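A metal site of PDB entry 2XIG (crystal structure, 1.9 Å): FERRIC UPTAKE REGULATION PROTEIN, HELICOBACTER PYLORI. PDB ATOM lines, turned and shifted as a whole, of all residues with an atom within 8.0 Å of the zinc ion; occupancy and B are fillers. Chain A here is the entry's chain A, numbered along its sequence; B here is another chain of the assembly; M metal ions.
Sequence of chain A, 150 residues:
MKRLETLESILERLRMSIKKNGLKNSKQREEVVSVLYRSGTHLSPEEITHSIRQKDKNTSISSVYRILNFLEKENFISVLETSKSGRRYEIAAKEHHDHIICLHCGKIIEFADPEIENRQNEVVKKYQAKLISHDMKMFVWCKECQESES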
ATOM      1  N   ILE A 101       5.529 -13.354  -6.416  1.00  0.00           N
ATOM      2  CA  ILE A 101       4.498 -13.447  -7.441  1.00  0.00           C
ATOM      3  C   ILE A 101       5.013 -12.944  -8.787  1.00  0.00           C
ATOM      4  O   ILE A 101       5.520 -11.834  -8.876  1.00  0.00           O
ATOM      5  CB  ILE A 101       3.239 -12.638  -7.109  1.00  0.00           C
ATOM      6  CG1 ILE A 101       2.719 -12.987  -5.716  1.00  0.00           C
ATOM      7  CG2 ILE A 101       2.180 -12.843  -8.186  1.00  0.00           C
ATOM      8  CD1 ILE A 101       3.179 -12.040  -4.637  1.00  0.00           C
ATOM      9  N   CYS A 102       4.861 -13.755  -9.826  1.00  0.00           N
ATOM     10  CA  CYS A 102       5.261 -13.325 -11.160  1.00  0.00           C
ATOM     11  C   CYS A 102       4.260 -12.344 -11.773  1.00  0.00           C
ATOM     12  O   CYS A 102       3.074 -12.632 -11.876  1.00  0.00           O
ATOM     13  CB  CYS A 102       5.459 -14.501 -12.093  1.00  0.00           C
ATOM     14  SG  CYS A 102       6.031 -13.963 -13.720  1.00  0.00           S
ATOM     15  N   LEU A 103       4.775 -11.191 -12.195  1.00  0.00           N
ATOM     16  CA  LEU A 103       3.957 -10.134 -12.764  1.00  0.00           C
ATOM     17  C   LEU A 103       3.376 -10.514 -14.121  1.00  0.00           C
ATOM     18  O   LEU A 103       2.375  -9.935 -14.555  1.00  0.00           O
ATOM     19  CB  LEU A 103       4.783  -8.862 -12.892  1.00  0.00           C
ATOM     20  CG  LEU A 103       4.991  -8.113 -11.583  1.00  0.00           C
ATOM     21  CD1 LEU A 103       6.199  -7.210 -11.662  1.00  0.00           C
ATOM     22  CD2 LEU A 103       3.732  -7.316 -11.224  1.00  0.00           C
ATOM     23  N   HIS A 104       3.988 -11.478 -14.795  1.00  0.00           N
ATOM     24  CA  HIS A 104       3.546 -11.850 -16.138  1.00  0.00           C
ATOM     25  C   HIS A 104       2.568 -13.033 -16.167  1.00  0.00           C
ATOM     26  O   HIS A 104       1.494 -12.934 -16.753  1.00  0.00           O
ATOM     27  CB  HIS A 104       4.749 -12.137 -17.045  1.00  0.00           C
ATOM     28  CG  HIS A 104       4.387 -12.357 -18.485  1.00  0.00           C
ATOM     29  ND1 HIS A 104       3.657 -11.433 -19.224  1.00  0.00           N
ATOM     30  CD2 HIS A 104       4.668 -13.375 -19.335  1.00  0.00           C
ATOM     31  CE1 HIS A 104       3.500 -11.884 -20.451  1.00  0.00           C
ATOM     32  NE2 HIS A 104       4.100 -13.057 -20.550  1.00  0.00           N
ATOM     33  N   CYS A 105       2.944 -14.135 -15.506  1.00  0.00           N
ATOM     34  CA  CYS A 105       2.119 -15.353 -15.519  1.00  0.00           C
ATOM     35  C   CYS A 105       1.291 -15.581 -14.244  1.00  0.00           C
ATOM     36  O   CYS A 105       0.369 -16.403 -14.229  1.00  0.00           O
ATOM     37  CB  CYS A 105       2.992 -16.577 -15.807  1.00  0.00           C
ATOM     38  SG  CYS A 105       4.044 -17.080 -14.438  1.00  0.00           S
ATOM     39  N   GLY A 106       1.610 -14.853 -13.178  1.00  0.00           N
ATOM     40  CA  GLY A 106       0.822 -14.940 -11.960  1.00  0.00           C
ATOM     41  C   GLY A 106       1.231 -16.064 -11.024  1.00  0.00           C
ATOM     42  O   GLY A 106       0.629 -16.267  -9.970  1.00  0.00           O
ATOM     43  N   LYS A 107       2.255 -16.802 -11.421  1.00  0.00           N
ATOM     44  CA  LYS A 107       2.786 -17.889 -10.612  1.00  0.00           C
ATOM     45  C   LYS A 107       3.165 -17.399  -9.204  1.00  0.00           C
ATOM     46  O   LYS A 107       3.726 -16.319  -9.044  1.00  0.00           O
ATOM     47  CB  LYS A 107       3.990 -18.497 -11.325  1.00  0.00           C
ATOM     48  CG  LYS A 107       5.020 -19.128 -10.432  1.00  0.00           C
ATOM     49  CD  LYS A 107       6.246 -19.482 -11.259  1.00  0.00           C
ATOM     50  CE  LYS A 107       5.864 -20.368 -12.431  1.00  0.00           C
ATOM     51  NZ  LYS A 107       7.064 -20.802 -13.185  1.00  0.00           N
ATOM     52  N   ILE A 108       2.830 -18.204  -8.195  1.00  0.00           N
ATOM     53  CA  ILE A 108       3.142 -17.869  -6.802  1.00  0.00           C
ATOM     54  C   ILE A 108       4.181 -18.821  -6.220  1.00  0.00           C
ATOM     55  O   ILE A 108       4.052 -20.031  -6.332  1.00  0.00           O
ATOM     56  CB  ILE A 108       1.871 -17.926  -5.931  1.00  0.00           C
ATOM     57  CG1 ILE A 108       0.817 -16.942  -6.443  1.00  0.00           C
ATOM     58  CG2 ILE A 108       2.195 -17.636  -4.459  1.00  0.00           C
ATOM     59  CD1 ILE A 108      -0.602 -17.223  -5.937  1.00  0.00           C
ATOM     60  N   VAL A 140       8.010 -10.264  -9.394  1.00  0.00           N
ATOM     61  CA  VAL A 140       9.159 -10.673 -10.192  1.00  0.00           C
ATOM     62  C   VAL A 140       8.798 -11.018 -11.622  1.00  0.00           C
ATOM     63  O   VAL A 140       7.622 -11.090 -11.978  1.00  0.00           O
ATOM     64  CB  VAL A 140       9.833 -11.935  -9.595  1.00  0.00           C
ATOM     65  CG1 VAL A 140      10.175 -11.733  -8.120  1.00  0.00           C
ATOM     66  CG2 VAL A 140       8.934 -13.157  -9.763  1.00  0.00           C
ATOM     67  N   TRP A 141       9.820 -11.233 -12.440  1.00  0.00           N
ATOM     68  CA  TRP A 141       9.681 -12.000 -13.669  1.00  0.00           C
ATOM     69  C   TRP A 141      10.285 -13.365 -13.372  1.00  0.00           C
ATOM     70  O   TRP A 141      11.479 -13.469 -13.085  1.00  0.00           O
ATOM     71  CB  TRP A 141      10.428 -11.358 -14.831  1.00  0.00           C
ATOM     72  CG  TRP A 141       9.975  -9.977 -15.177  1.00  0.00           C
ATOM     73  CD1 TRP A 141       8.813  -9.365 -14.803  1.00  0.00           C
ATOM     74  CD2 TRP A 141      10.665  -9.045 -16.019  1.00  0.00           C
ATOM     75  NE1 TRP A 141       8.759  -8.100 -15.336  1.00  0.00           N
ATOM     76  CE2 TRP A 141       9.881  -7.881 -16.089  1.00  0.00           C
ATOM     77  CE3 TRP A 141      11.888  -9.075 -16.711  1.00  0.00           C
ATOM     78  CZ2 TRP A 141      10.268  -6.756 -16.819  1.00  0.00           C
ATOM     79  CZ3 TRP A 141      12.266  -7.968 -17.428  1.00  0.00           C
ATOM     80  CH2 TRP A 141      11.463  -6.823 -17.483  1.00  0.00           C
ATOM     81  N   CYS A 142       9.455 -14.405 -13.413  1.00  0.00           N
ATOM     82  CA  CYS A 142       9.913 -15.740 -13.046  1.00  0.00           C
ATOM     83  C   CYS A 142      10.799 -16.362 -14.115  1.00  0.00           C
ATOM     84  O   CYS A 142      10.840 -15.911 -15.262  1.00  0.00           O
ATOM     85  CB  CYS A 142       8.729 -16.660 -12.756  1.00  0.00           C
ATOM     86  SG  CYS A 142       7.981 -17.378 -14.233  1.00  0.00           S
ATOM     87  N   LYS A 143      11.522 -17.411 -13.730  1.00  0.00           N
ATOM     88  CA  LYS A 143      12.476 -18.070 -14.607  1.00  0.00           C
ATOM     89  C   LYS A 143      11.862 -18.425 -15.953  1.00  0.00           C
ATOM     90  O   LYS A 143      12.471 -18.199 -16.985  1.00  0.00           O
ATOM     91  CB  LYS A 143      13.016 -19.327 -13.930  1.00  0.00           C
ATOM     92  CG  LYS A 143      13.537 -20.399 -14.873  1.00  0.00           C
ATOM     93  CD  LYS A 143      15.043 -20.318 -15.065  1.00  0.00           C
ATOM     94  CE  LYS A 143      15.531 -21.539 -15.833  1.00  0.00           C
ATOM     95  NZ  LYS A 143      17.008 -21.632 -15.895  1.00  0.00           N
ATOM     96  N   GLU A 144      10.653 -18.958 -15.936  1.00  0.00           N
ATOM     97  CA  GLU A 144      10.019 -19.476 -17.147  1.00  0.00           C
ATOM     98  C   GLU A 144       9.531 -18.372 -18.081  1.00  0.00           C
ATOM     99  O   GLU A 144       9.508 -18.536 -19.299  1.00  0.00           O
ATOM    100  CB  GLU A 144       8.863 -20.409 -16.775  1.00  0.00           C
ATOM    101  CG  GLU A 144       9.314 -21.749 -16.202  1.00  0.00           C
ATOM    102  CD  GLU A 144       9.907 -21.628 -14.809  1.00  0.00           C
ATOM    103  OE1 GLU A 144       9.508 -20.705 -14.067  1.00  0.00           O
ATOM    104  OE2 GLU A 144      10.764 -22.478 -14.443  1.00  0.00           O
ATOM    105  N   CYS A 145       9.148 -17.243 -17.498  1.00  0.00           N
ATOM    106  CA  CYS A 145       8.646 -16.136 -18.298  1.00  0.00           C
ATOM    107  C   CYS A 145       9.802 -15.422 -18.990  1.00  0.00           C
ATOM    108  O   CYS A 145       9.638 -14.843 -20.077  1.00  0.00           O
ATOM    109  CB  CYS A 145       7.827 -15.178 -17.439  1.00  0.00           C
ATOM    110  SG  CYS A 145       6.150 -15.751 -17.152  1.00  0.00           S
ATOM    111  N   GLN A 146      10.980 -15.470 -18.370  1.00  0.00           N
ATOM    112  CA  GLN A 146      12.156 -14.821 -18.916  1.00  0.00           C
ATOM    113  C   GLN A 146      12.791 -15.629 -20.046  1.00  0.00           C
ATOM    114  O   GLN A 146      13.535 -15.091 -20.860  1.00  0.00           O
ATOM    115  CB  GLN A 146      13.181 -14.578 -17.810  1.00  0.00           C
ATOM    116  CG  GLN A 146      12.769 -13.499 -16.832  1.00  0.00           C
ATOM    117  CD  GLN A 146      13.903 -13.043 -15.949  1.00  0.00           C
ATOM    118  OE1 GLN A 146      14.194 -13.667 -14.927  1.00  0.00           O
ATOM    119  NE2 GLN A 146      14.552 -11.949 -16.333  1.00  0.00           N
ATOM    120  N   TRP B 141       9.461  -6.351 -22.896  1.00  0.00           N
ATOM    121  CA  TRP B 141      10.660  -6.269 -22.073  1.00  0.00           C
ATOM    122  C   TRP B 141      11.827  -6.243 -23.046  1.00  0.00           C
ATOM    123  O   TRP B 141      12.009  -7.185 -23.818  1.00  0.00           O
ATOM    124  CB  TRP B 141      10.796  -7.481 -21.154  1.00  0.00           C
ATOM    125  CG  TRP B 141       9.624  -7.749 -20.281  1.00  0.00           C
ATOM    126  CD1 TRP B 141       8.630  -6.863 -19.959  1.00  0.00           C
ATOM    127  CD2 TRP B 141       9.318  -8.973 -19.606  1.00  0.00           C
ATOM    128  NE1 TRP B 141       7.721  -7.470 -19.131  1.00  0.00           N
ATOM    129  CE2 TRP B 141       8.119  -8.764 -18.889  1.00  0.00           C
ATOM    130  CE3 TRP B 141       9.939 -10.227 -19.522  1.00  0.00           C
ATOM    131  CZ2 TRP B 141       7.527  -9.758 -18.108  1.00  0.00           C
ATOM    132  CZ3 TRP B 141       9.348 -11.216 -18.750  1.00  0.00           C
ATOM    133  CH2 TRP B 141       8.156 -10.976 -18.052  1.00  0.00           C
HETATM  134 ZN    ZN M   1       6.087 -16.070 -14.824  1.00  0.00          ZN
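The side-chain sulfur (SG) of Cys 105 is bound to the zinc ion (2.3 Å).
The zinc ion is bound by the side-chain sulfur (SG) of Cys 145 (2.4 Å).
The side-chain sulfur (SG) of Cys 142 is bound to the zinc ion.
The zinc ion is bound by SG of Cys 102, at 2.4 Å.
The zinc ion has four donor atoms within binding distance.
SG of Cys 105 sits close to N of Lys 107 (3.5 Å).
The side-chain sulfur (SG) of Cys 142 lies close to the side-chain amino group (NZ) of Lys 107, 3.7 Å away.
N of Glu 144 lies close to SG of Cys 142 (3.5 Å).
The backbone NH of His 104 sits close to the side-chain sulfur of Cys 102 (3.4 Å).
N of Cys 102 sits at hydrogen-bond distance from O of Lys 107, at 2.9 Å.
SG of Cys 102 sits close to O of Val 140 (3.7 Å).
Within 4 Å of the zinc ion: Cys 102, Cys 105, Cys 142 and Cys 145.
Along chain A the residues within 4 Å of the zinc ion span positions 102 to 145.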
